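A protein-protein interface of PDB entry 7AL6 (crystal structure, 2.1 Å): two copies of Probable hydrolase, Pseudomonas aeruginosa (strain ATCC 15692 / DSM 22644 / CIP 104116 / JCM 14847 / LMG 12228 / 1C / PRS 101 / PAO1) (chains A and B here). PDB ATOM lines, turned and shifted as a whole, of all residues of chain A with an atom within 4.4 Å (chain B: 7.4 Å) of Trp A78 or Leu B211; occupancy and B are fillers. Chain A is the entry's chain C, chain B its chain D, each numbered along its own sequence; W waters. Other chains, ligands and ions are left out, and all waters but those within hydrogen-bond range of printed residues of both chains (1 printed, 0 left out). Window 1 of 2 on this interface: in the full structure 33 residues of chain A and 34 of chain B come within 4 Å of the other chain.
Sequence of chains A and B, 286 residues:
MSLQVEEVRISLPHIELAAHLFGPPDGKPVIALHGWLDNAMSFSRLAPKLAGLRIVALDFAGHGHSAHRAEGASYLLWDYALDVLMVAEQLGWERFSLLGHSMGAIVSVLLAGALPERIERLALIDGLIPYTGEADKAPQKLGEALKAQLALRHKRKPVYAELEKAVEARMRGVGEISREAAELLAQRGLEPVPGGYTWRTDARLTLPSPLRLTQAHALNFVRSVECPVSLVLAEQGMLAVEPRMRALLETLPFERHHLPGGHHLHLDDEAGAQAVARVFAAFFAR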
ATOM      1  N   LEU A  76      18.837 -21.931 -25.838  1.00  0.00           N
ATOM      2  CA  LEU A  76      17.467 -21.898 -26.408  1.00  0.00           C
ATOM      3  C   LEU A  76      17.013 -20.450 -26.527  1.00  0.00           C
ATOM      4  O   LEU A  76      17.565 -19.605 -25.867  1.00  0.00           O
ATOM      5  CB  LEU A  76      16.527 -22.738 -25.560  1.00  0.00           C
ATOM      6  CG  LEU A  76      16.985 -24.169 -25.370  1.00  0.00           C
ATOM      7  CD1 LEU A  76      15.926 -24.977 -24.678  1.00  0.00           C
ATOM      8  CD2 LEU A  76      17.377 -24.793 -26.688  1.00  0.00           C
ATOM      9  N   LEU A  77      16.014 -20.205 -27.350  1.00  0.00           N
ATOM     10  CA  LEU A  77      15.579 -18.844 -27.642  1.00  0.00           C
ATOM     11  C   LEU A  77      15.154 -18.113 -26.385  1.00  0.00           C
ATOM     12  O   LEU A  77      15.447 -16.922 -26.223  1.00  0.00           O
ATOM     13  CB  LEU A  77      14.430 -18.862 -28.647  1.00  0.00           C
ATOM     14  CG  LEU A  77      14.812 -19.205 -30.090  1.00  0.00           C
ATOM     15  CD1 LEU A  77      13.595 -19.422 -30.923  1.00  0.00           C
ATOM     16  CD2 LEU A  77      15.631 -18.122 -30.690  1.00  0.00           C
ATOM     17  N   TRP A  78      14.412 -18.783 -25.523  1.00  0.00           N
ATOM     18  CA  TRP A  78      13.953 -18.163 -24.302  1.00  0.00           C
ATOM     19  C   TRP A  78      15.054 -18.042 -23.253  1.00  0.00           C
ATOM     20  O   TRP A  78      14.850 -17.323 -22.263  1.00  0.00           O
ATOM     21  CB  TRP A  78      12.782 -18.937 -23.697  1.00  0.00           C
ATOM     22  CG  TRP A  78      12.995 -20.395 -23.601  1.00  0.00           C
ATOM     23  CD1 TRP A  78      13.580 -21.087 -22.579  1.00  0.00           C
ATOM     24  CD2 TRP A  78      12.601 -21.362 -24.576  1.00  0.00           C
ATOM     25  NE1 TRP A  78      13.592 -22.439 -22.883  1.00  0.00           N
ATOM     26  CE2 TRP A  78      12.985 -22.627 -24.098  1.00  0.00           C
ATOM     27  CE3 TRP A  78      12.013 -21.271 -25.840  1.00  0.00           C
ATOM     28  CZ2 TRP A  78      12.762 -23.800 -24.825  1.00  0.00           C
ATOM     29  CZ3 TRP A  78      11.764 -22.446 -26.547  1.00  0.00           C
ATOM     30  CH2 TRP A  78      12.154 -23.683 -26.045  1.00  0.00           C
ATOM     31  N   ASP A  79      16.218 -18.691 -23.447  1.00  0.00           N
ATOM     32  CA  ASP A  79      17.365 -18.377 -22.590  1.00  0.00           C
ATOM     33  C   ASP A  79      17.909 -16.993 -22.937  1.00  0.00           C
ATOM     34  O   ASP A  79      18.182 -16.187 -22.047  1.00  0.00           O
ATOM     35  CB  ASP A  79      18.483 -19.413 -22.723  1.00  0.00           C
ATOM     36  CG  ASP A  79      18.042 -20.825 -22.329  1.00  0.00           C
ATOM     37  OD1 ASP A  79      17.388 -20.997 -21.300  1.00  0.00           O
ATOM     38  OD2 ASP A  79      18.357 -21.785 -23.076  1.00  0.00           O
ATOM     39  N   TYR A  80      18.074 -16.701 -24.232  1.00  0.00           N
ATOM     40  CA  TYR A  80      18.421 -15.340 -24.640  1.00  0.00           C
ATOM     41  C   TYR A  80      17.395 -14.329 -24.140  1.00  0.00           C
ATOM     42  O   TYR A  80      17.753 -13.225 -23.711  1.00  0.00           O
ATOM     43  CB  TYR A  80      18.508 -15.239 -26.168  1.00  0.00           C
ATOM     44  CG  TYR A  80      19.540 -16.084 -26.858  1.00  0.00           C
ATOM     45  CD1 TYR A  80      20.885 -15.999 -26.526  1.00  0.00           C
ATOM     46  CD2 TYR A  80      19.174 -16.942 -27.867  1.00  0.00           C
ATOM     47  CE1 TYR A  80      21.822 -16.725 -27.215  1.00  0.00           C
ATOM     48  CE2 TYR A  80      20.093 -17.713 -28.520  1.00  0.00           C
ATOM     49  CZ  TYR A  80      21.421 -17.596 -28.185  1.00  0.00           C
ATOM     50  OH  TYR A  80      22.351 -18.339 -28.848  1.00  0.00           O
ATOM     51  N   ALA A  81      16.108 -14.661 -24.185  1.00  0.00           N
ATOM     52  CA  ALA A  81      15.024 -13.745 -23.776  1.00  0.00           C
ATOM     53  C   ALA A  81      15.221 -13.359 -22.310  1.00  0.00           C
ATOM     54  O   ALA A  81      15.143 -12.204 -22.019  1.00  0.00           O
ATOM     55  CB  ALA A  81      13.684 -14.374 -23.987  1.00  0.00           C
ATOM     56  N   LEU A  82      15.522 -14.318 -21.453  1.00  0.00           N
ATOM     57  CA  LEU A  82      15.772 -14.067 -20.018  1.00  0.00           C
ATOM     58  C   LEU A  82      17.009 -13.177 -19.861  1.00  0.00           C
ATOM     59  O   LEU A  82      16.939 -12.256 -19.105  1.00  0.00           O
ATOM     60  CB  LEU A  82      15.948 -15.378 -19.256  1.00  0.00           C
ATOM     61  CG  LEU A  82      16.240 -15.172 -17.777  1.00  0.00           C
ATOM     62  CD1 LEU A  82      15.111 -14.407 -17.122  1.00  0.00           C
ATOM     63  CD2 LEU A  82      16.495 -16.478 -17.072  1.00  0.00           C
ATOM     64  N   LEU A 211      13.051 -29.190 -28.077  1.00  0.00           N
ATOM     65  CA  LEU A 211      11.610 -28.966 -28.128  1.00  0.00           C
ATOM     66  C   LEU A 211      11.367 -27.683 -28.918  1.00  0.00           C
ATOM     67  O   LEU A 211      11.567 -26.586 -28.400  1.00  0.00           O
ATOM     68  CB  LEU A 211      11.016 -28.868 -26.739  1.00  0.00           C
ATOM     69  CG  LEU A 211       9.507 -28.612 -26.759  1.00  0.00           C
ATOM     70  CD1 LEU A 211       8.695 -29.732 -27.408  1.00  0.00           C
ATOM     71  CD2 LEU A 211       9.065 -28.425 -25.348  1.00  0.00           C
ATOM     72  N   LEU A 213       9.047 -24.847 -30.864  1.00  0.00           N
ATOM     73  CA  LEU A 213       7.738 -24.177 -30.784  1.00  0.00           C
ATOM     74  C   LEU A 213       6.893 -24.793 -31.897  1.00  0.00           C
ATOM     75  O   LEU A 213       7.409 -24.974 -32.965  1.00  0.00           O
ATOM     76  CB  LEU A 213       7.908 -22.680 -31.044  1.00  0.00           C
ATOM     77  CG  LEU A 213       8.371 -21.810 -29.884  1.00  0.00           C
ATOM     78  CD1 LEU A 213       8.197 -20.356 -30.234  1.00  0.00           C
ATOM     79  CD2 LEU A 213       7.606 -22.130 -28.629  1.00  0.00           C
ATOM     80  N   HIS A 217       2.214 -22.263 -31.446  1.00  0.00           N
ATOM     81  CA  HIS A 217       2.962 -21.433 -30.480  1.00  0.00           C
ATOM     82  C   HIS A 217       3.448 -20.126 -31.126  1.00  0.00           C
ATOM     83  O   HIS A 217       3.251 -19.031 -30.591  1.00  0.00           O
ATOM     84  CB  HIS A 217       4.154 -22.229 -29.933  1.00  0.00           C
ATOM     85  CG  HIS A 217       3.788 -23.197 -28.855  1.00  0.00           C
ATOM     86  ND1 HIS A 217       3.528 -24.528 -29.109  1.00  0.00           N
ATOM     87  CD2 HIS A 217       3.611 -23.029 -27.529  1.00  0.00           C
ATOM     88  CE1 HIS A 217       3.224 -25.140 -27.978  1.00  0.00           C
ATOM     89  NE2 HIS A 217       3.277 -24.258 -26.998  1.00  0.00           N
ATOM     90  N   SER B  74      19.036 -24.986 -16.558  1.00  0.00           N
ATOM     91  CA  SER B  74      17.642 -25.278 -16.209  1.00  0.00           C
ATOM     92  C   SER B  74      17.453 -26.685 -15.600  1.00  0.00           C
ATOM     93  O   SER B  74      18.271 -27.604 -15.786  1.00  0.00           O
ATOM     94  CB  SER B  74      16.787 -25.168 -17.469  1.00  0.00           C
ATOM     95  OG  SER B  74      17.343 -25.950 -18.542  1.00  0.00           O
ATOM     96  N   LEU B  76      14.666 -28.653 -16.545  1.00  0.00           N
ATOM     97  CA  LEU B  76      13.546 -29.106 -17.400  1.00  0.00           C
ATOM     98  C   LEU B  76      13.583 -30.635 -17.478  1.00  0.00           C
ATOM     99  O   LEU B  76      14.619 -31.204 -17.205  1.00  0.00           O
ATOM    100  CB  LEU B  76      13.626 -28.416 -18.757  1.00  0.00           C
ATOM    101  CG  LEU B  76      13.609 -26.895 -18.695  1.00  0.00           C
ATOM    102  CD1 LEU B  76      13.588 -26.279 -20.067  1.00  0.00           C
ATOM    103  CD2 LEU B  76      12.442 -26.403 -17.869  1.00  0.00           C
ATOM    104  N   TRP B  78      13.706 -32.767 -19.887  1.00  0.00           N
ATOM    105  CA  TRP B  78      14.655 -33.368 -20.813  1.00  0.00           C
ATOM    106  C   TRP B  78      16.106 -33.090 -20.448  1.00  0.00           C
ATOM    107  O   TRP B  78      17.004 -33.743 -21.011  1.00  0.00           O
ATOM    108  CB  TRP B  78      14.403 -32.886 -22.247  1.00  0.00           C
ATOM    109  CG  TRP B  78      14.261 -31.421 -22.354  1.00  0.00           C
ATOM    110  CD1 TRP B  78      15.254 -30.507 -22.498  1.00  0.00           C
ATOM    111  CD2 TRP B  78      13.042 -30.691 -22.350  1.00  0.00           C
ATOM    112  NE1 TRP B  78      14.731 -29.247 -22.577  1.00  0.00           N
ATOM    113  CE2 TRP B  78      13.371 -29.332 -22.480  1.00  0.00           C
ATOM    114  CE3 TRP B  78      11.700 -31.057 -22.257  1.00  0.00           C
ATOM    115  CZ2 TRP B  78      12.415 -28.336 -22.507  1.00  0.00           C
ATOM    116  CZ3 TRP B  78      10.745 -30.064 -22.280  1.00  0.00           C
ATOM    117  CH2 TRP B  78      11.106 -28.721 -22.404  1.00  0.00           C
ATOM    118  N   GLY B 133       0.358 -27.837 -21.341  1.00  0.00           N
ATOM    119  CA  GLY B 133      -0.134 -26.496 -21.578  1.00  0.00           C
ATOM    120  C   GLY B 133      -0.256 -26.259 -23.068  1.00  0.00           C
ATOM    121  O   GLY B 133       0.590 -26.711 -23.841  1.00  0.00           O
ATOM    122  N   GLU B 134      -1.317 -25.583 -23.501  1.00  0.00           N
ATOM    123  CA  GLU B 134      -1.544 -25.416 -24.923  1.00  0.00           C
ATOM    124  C   GLU B 134      -0.950 -24.109 -25.413  1.00  0.00           C
ATOM    125  O   GLU B 134      -0.552 -23.237 -24.637  1.00  0.00           O
ATOM    126  CB  GLU B 134      -3.041 -25.471 -25.265  1.00  0.00           C
ATOM    127  CG  GLU B 134      -3.690 -26.820 -24.911  1.00  0.00           C
ATOM    128  CD  GLU B 134      -2.924 -28.032 -25.470  1.00  0.00           C
ATOM    129  OE1 GLU B 134      -2.857 -28.170 -26.706  1.00  0.00           O
ATOM    130  OE2 GLU B 134      -2.391 -28.824 -24.663  1.00  0.00           O
ATOM    131  N   ALA B 135      -0.889 -23.992 -26.740  1.00  0.00           N
ATOM    132  CA  ALA B 135      -0.213 -22.866 -27.361  1.00  0.00           C
ATOM    133  C   ALA B 135      -0.870 -21.541 -26.989  1.00  0.00           C
ATOM    134  O   ALA B 135      -0.191 -20.507 -26.949  1.00  0.00           O
ATOM    135  CB  ALA B 135      -0.207 -23.051 -28.878  1.00  0.00           C
ATOM    136  N   ALA B 138       0.742 -20.085 -24.015  1.00  0.00           N
ATOM    137  CA  ALA B 138       2.207 -20.202 -23.998  1.00  0.00           C
ATOM    138  C   ALA B 138       2.887 -18.842 -23.826  1.00  0.00           C
ATOM    139  O   ALA B 138       3.804 -18.733 -23.019  1.00  0.00           O
ATOM    140  CB  ALA B 138       2.702 -20.900 -25.269  1.00  0.00           C
ATOM    141  N   PRO B 139       2.461 -17.749 -24.480  1.00  0.00           N
ATOM    142  CA  PRO B 139       3.090 -16.462 -24.245  1.00  0.00           C
ATOM    143  C   PRO B 139       2.980 -16.073 -22.762  1.00  0.00           C
ATOM    144  O   PRO B 139       3.916 -15.644 -22.196  1.00  0.00           O
ATOM    145  CB  PRO B 139       2.299 -15.516 -25.147  1.00  0.00           C
ATOM    146  CG  PRO B 139       1.822 -16.402 -26.236  1.00  0.00           C
ATOM    147  CD  PRO B 139       1.503 -17.709 -25.552  1.00  0.00           C
ATOM    148  N   LYS B 141       2.562 -18.143 -20.148  1.00  0.00           N
ATOM    149  CA  LYS B 141       3.367 -19.078 -19.333  1.00  0.00           C
ATOM    150  C   LYS B 141       4.838 -18.656 -19.413  1.00  0.00           C
ATOM    151  O   LYS B 141       5.472 -18.679 -18.403  1.00  0.00           O
ATOM    152  CB  LYS B 141       3.082 -20.531 -19.705  1.00  0.00           C
ATOM    153  CG  LYS B 141       1.875 -21.136 -18.993  1.00  0.00           C
ATOM    154  CD  LYS B 141       1.544 -22.545 -19.459  1.00  0.00           C
ATOM    155  CE  LYS B 141       0.263 -23.119 -18.888  1.00  0.00           C
ATOM    156  NZ  LYS B 141      -0.771 -23.329 -19.920  1.00  0.00           N
ATOM    157  N   LEU B 142       5.329 -18.239 -20.570  1.00  0.00           N
ATOM    158  CA  LEU B 142       6.725 -17.798 -20.678  1.00  0.00           C
ATOM    159  C   LEU B 142       6.945 -16.539 -19.860  1.00  0.00           C
ATOM    160  O   LEU B 142       7.943 -16.423 -19.138  1.00  0.00           O
ATOM    161  CB  LEU B 142       7.125 -17.542 -22.141  1.00  0.00           C
ATOM    162  CG  LEU B 142       8.528 -16.902 -22.318  1.00  0.00           C
ATOM    163  CD1 LEU B 142       9.549 -17.838 -21.697  1.00  0.00           C
ATOM    164  CD2 LEU B 142       8.897 -16.591 -23.750  1.00  0.00           C
ATOM    165  N   ALA B 145       7.333 -17.564 -16.371  1.00  0.00           N
ATOM    166  CA  ALA B 145       8.647 -18.149 -16.095  1.00  0.00           C
ATOM    167  C   ALA B 145       9.739 -17.075 -16.039  1.00  0.00           C
ATOM    168  O   ALA B 145      10.594 -17.108 -15.154  1.00  0.00           O
ATOM    169  CB  ALA B 145       8.988 -19.208 -17.149  1.00  0.00           C
ATOM    170  N   LEU B 146       9.731 -16.122 -16.978  1.00  0.00           N
ATOM    171  CA  LEU B 146      10.722 -15.052 -16.955  1.00  0.00           C
ATOM    172  C   LEU B 146      10.612 -14.212 -15.693  1.00  0.00           C
ATOM    173  O   LEU B 146      11.622 -13.889 -15.065  1.00  0.00           O
ATOM    174  CB  LEU B 146      10.585 -14.167 -18.178  1.00  0.00           C
ATOM    175  CG  LEU B 146      10.872 -14.853 -19.529  1.00  0.00           C
ATOM    176  CD1 LEU B 146      10.423 -13.907 -20.616  1.00  0.00           C
ATOM    177  CD2 LEU B 146      12.343 -15.219 -19.652  1.00  0.00           C
ATOM    178  N   GLN B 149      12.079 -16.113 -12.799  1.00  0.00           N
ATOM    179  CA  GLN B 149      13.540 -16.124 -12.792  1.00  0.00           C
ATOM    180  C   GLN B 149      14.075 -14.853 -12.164  1.00  0.00           C
ATOM    181  O   GLN B 149      15.019 -14.891 -11.377  1.00  0.00           O
ATOM    182  CB  GLN B 149      14.088 -16.272 -14.216  1.00  0.00           C
ATOM    183  CG  GLN B 149      13.774 -17.590 -14.854  1.00  0.00           C
ATOM    184  CD  GLN B 149      14.892 -18.577 -14.614  1.00  0.00           C
ATOM    185  OE1 GLN B 149      15.723 -18.376 -13.722  1.00  0.00           O
ATOM    186  NE2 GLN B 149      14.958 -19.615 -15.441  1.00  0.00           N
ATOM    187  N   PRO B 208       8.718 -22.263 -12.839  1.00  0.00           N
ATOM    188  CA  PRO B 208       7.823 -22.848 -13.815  1.00  0.00           C
ATOM    189  C   PRO B 208       8.530 -23.017 -15.163  1.00  0.00           C
ATOM    190  O   PRO B 208       9.363 -22.231 -15.473  1.00  0.00           O
ATOM    191  CB  PRO B 208       6.670 -21.854 -13.863  1.00  0.00           C
ATOM    192  CG  PRO B 208       7.309 -20.560 -13.556  1.00  0.00           C
ATOM    193  CD  PRO B 208       8.403 -20.879 -12.572  1.00  0.00           C
ATOM    194  N   SER B 209       8.180 -24.049 -15.918  1.00  0.00           N
ATOM    195  CA  SER B 209       8.808 -24.283 -17.201  1.00  0.00           C
ATOM    196  C   SER B 209       8.515 -23.100 -18.120  1.00  0.00           C
ATOM    197  O   SER B 209       7.424 -22.515 -18.046  1.00  0.00           O
ATOM    198  CB  SER B 209       8.308 -25.574 -17.828  1.00  0.00           C
ATOM    199  OG  SER B 209       8.781 -25.667 -19.166  1.00  0.00           O
ATOM    200  N   PRO B 210       9.462 -22.708 -18.978  1.00  0.00           N
ATOM    201  CA  PRO B 210       9.160 -21.664 -19.976  1.00  0.00           C
ATOM    202  C   PRO B 210       8.304 -22.147 -21.141  1.00  0.00           C
ATOM    203  O   PRO B 210       7.789 -21.309 -21.905  1.00  0.00           O
ATOM    204  CB  PRO B 210      10.547 -21.245 -20.477  1.00  0.00           C
ATOM    205  CG  PRO B 210      11.359 -22.624 -20.367  1.00  0.00           C
ATOM    206  CD  PRO B 210      10.862 -23.175 -19.060  1.00  0.00           C
ATOM    207  N   LEU B 211       8.201 -23.460 -21.334  1.00  0.00           N
ATOM    208  CA  LEU B 211       7.459 -24.041 -22.454  1.00  0.00           C
ATOM    209  C   LEU B 211       6.999 -25.433 -22.048  1.00  0.00           C
ATOM    210  O   LEU B 211       7.810 -26.362 -21.940  1.00  0.00           O
ATOM    211  CB  LEU B 211       8.316 -24.105 -23.696  1.00  0.00           C
ATOM    212  CG  LEU B 211       7.549 -24.641 -24.911  1.00  0.00           C
ATOM    213  CD1 LEU B 211       6.423 -23.724 -25.366  1.00  0.00           C
ATOM    214  CD2 LEU B 211       8.535 -24.850 -26.036  1.00  0.00           C
ATOM    215  N   ARG B 212       5.716 -25.573 -21.795  1.00  0.00           N
ATOM    216  CA  ARG B 212       5.127 -26.865 -21.412  1.00  0.00           C
ATOM    217  C   ARG B 212       4.936 -27.729 -22.655  1.00  0.00           C
ATOM    218  O   ARG B 212       4.818 -27.204 -23.730  1.00  0.00           O
ATOM    219  CB  ARG B 212       3.787 -26.664 -20.707  1.00  0.00           C
ATOM    220  CG  ARG B 212       3.900 -26.376 -19.220  1.00  0.00           C
ATOM    221  CD  ARG B 212       2.553 -26.262 -18.547  1.00  0.00           C
ATOM    222  NE  ARG B 212       2.663 -26.297 -17.107  1.00  0.00           N
ATOM    223  CZ  ARG B 212       1.644 -26.225 -16.261  1.00  0.00           C
ATOM    224  NH1 ARG B 212       0.408 -26.100 -16.707  1.00  0.00           N
ATOM    225  NH2 ARG B 212       1.865 -26.272 -14.963  1.00  0.00           N
ATOM    226  N   LEU B 213       4.915 -29.037 -22.480  1.00  0.00           N
ATOM    227  CA  LEU B 213       4.526 -29.947 -23.563  1.00  0.00           C
ATOM    228  C   LEU B 213       3.029 -29.726 -23.777  1.00  0.00           C
ATOM    229  O   LEU B 213       2.330 -29.593 -22.801  1.00  0.00           O
ATOM    230  CB  LEU B 213       4.796 -31.382 -23.126  1.00  0.00           C
ATOM    231  CG  LEU B 213       6.232 -31.853 -23.260  1.00  0.00           C
ATOM    232  CD1 LEU B 213       6.308 -33.350 -23.129  1.00  0.00           C
ATOM    233  CD2 LEU B 213       6.797 -31.410 -24.577  1.00  0.00           C
ATOM    234  N   THR B 214       2.545 -29.695 -25.011  1.00  0.00           N
ATOM    235  CA  THR B 214       1.087 -29.659 -25.289  1.00  0.00           C
ATOM    236  C   THR B 214       0.522 -31.074 -25.104  1.00  0.00           C
ATOM    237  O   THR B 214       1.283 -32.021 -25.126  1.00  0.00           O
ATOM    238  CB  THR B 214       0.720 -29.176 -26.689  1.00  0.00           C
ATOM    239  OG1 THR B 214       1.001 -30.256 -27.562  1.00  0.00           O
ATOM    240  CG2 THR B 214       1.441 -27.925 -27.131  1.00  0.00           C
ATOM    241  N   HIS B 217       1.815 -33.314 -27.626  1.00  0.00           N
ATOM    242  CA  HIS B 217       3.182 -33.736 -27.332  1.00  0.00           C
ATOM    243  C   HIS B 217       3.183 -34.936 -26.405  1.00  0.00           C
ATOM    244  O   HIS B 217       3.812 -35.957 -26.693  1.00  0.00           O
ATOM    245  CB  HIS B 217       3.986 -32.581 -26.699  1.00  0.00           C
ATOM    246  CG  HIS B 217       4.456 -31.557 -27.686  1.00  0.00           C
ATOM    247  ND1 HIS B 217       3.800 -30.363 -27.891  1.00  0.00           N
ATOM    248  CD2 HIS B 217       5.531 -31.537 -28.506  1.00  0.00           C
ATOM    249  CE1 HIS B 217       4.452 -29.653 -28.794  1.00  0.00           C
ATOM    250  NE2 HIS B 217       5.501 -30.349 -29.194  1.00  0.00           N
HETATM  251  O   HOH W   1       2.817 -25.257 -24.672  1.00  0.00           O
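Water W1 lies within hydrogen-bond range of a ring nitrogen (NE2) of His A217 (2.6 Å), the backbone carbonyl oxygen of Gly B133 (2.8 Å) and the backbone carbonyl oxygen of Arg B212 (2.9 Å).
Trp A78 touches Leu B211, and with the chains exchanged Leu A211 touches Trp B78.
Leu B211 touches its own counterpart, Leu A211.
Leu A211 touches Leu B213, and with the chains exchanged Leu A213 touches Leu B211.
Leu A211 touches His B217, and with the chains exchanged His A217 touches Leu B211.
Of the 14 pairs that touch across the chains among the printed residues, 7 have their exchanged pair printed and touching as well.
Printed residues of chain A that touch a printed residue of chain B: Trp A78, Leu A82, Leu A211, Leu A213 and His A217.
Hydrophobic or aromatic side chains of chain A that line the printed part of chain B: Trp A78, Leu A82, Leu A211, Leu A213 and His A217.
Along chain A the printed residues that touch a printed residue of chain B span positions 78 to 217.
Of the 21 printed residues of chain B, 11 touch a printed residue of chain A.
Hydrophobic or aromatic side chains of chain B that line the printed part of chain A: Trp B78, Ala B135, Ala B138, Leu B142, Leu B146, Pro B210, Leu B211, Leu B213 and His B217.
Among the printed residues, 14 pairs touch across the chains.
Among the printed residues, no Asp or Glu carboxylate lies within 4 Å of a Lys or Arg side-chain nitrogen of the other chain.
The backbone NH of Gly B133 is in hydrogen-bond range of the backbone carbonyl oxygen of Leu B213, at 3.0 Å.
The side-chain hydroxyl (OG) of Ser B209 lies within hydrogen-bond range of the backbone carbonyl oxygen (O) of Leu B211.
ND1 of His B217 is in hydrogen-bond range of OG1 of Thr B214.
Trp A78 touches Leu B142 (CB to CD1, 3.96 Å).
CG of Pro B210 touches NE1 of Trp A78 (3.4 Å).
CB of Leu A82 touches CD2 of Leu B146 (3.6 Å).
Trp B78 touches Leu A211.
CD2 of Leu B211 touches CD2 of Leu A211, 3.7 Å away.
Leu A211 touches Leu B213.
Leu A213 touches Leu B211.
His A217 touches Ala B138.
His A217 touches Leu B211.
His A217 touches Thr B214.
Of the printed residues of chain B, Trp A78 touches Leu B142 (3.96 Å), Pro B210 (3.4 Å) and Leu B211 (3.8 Å).
Leu B211 touches four residues of chain A.
Printed residues of chain A within 4 Å of Thr B214: His A217 (3.4 Å).
Of the printed residues of chain A, Ala B135 touches His A217.
Printed residues of chain A within 4 Å of Leu B213: Leu A211.
Of the printed residues of chain A, Leu B142 touches Trp A78.
Of the printed residues of chain A, Leu B146 touches Leu A82 (3.6 Å).
Gly B133 touches none of the printed residues of chain A.
The nearest printed residue of chain A that does not touch Ala B138 is Leu A213 (6.1 Å).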
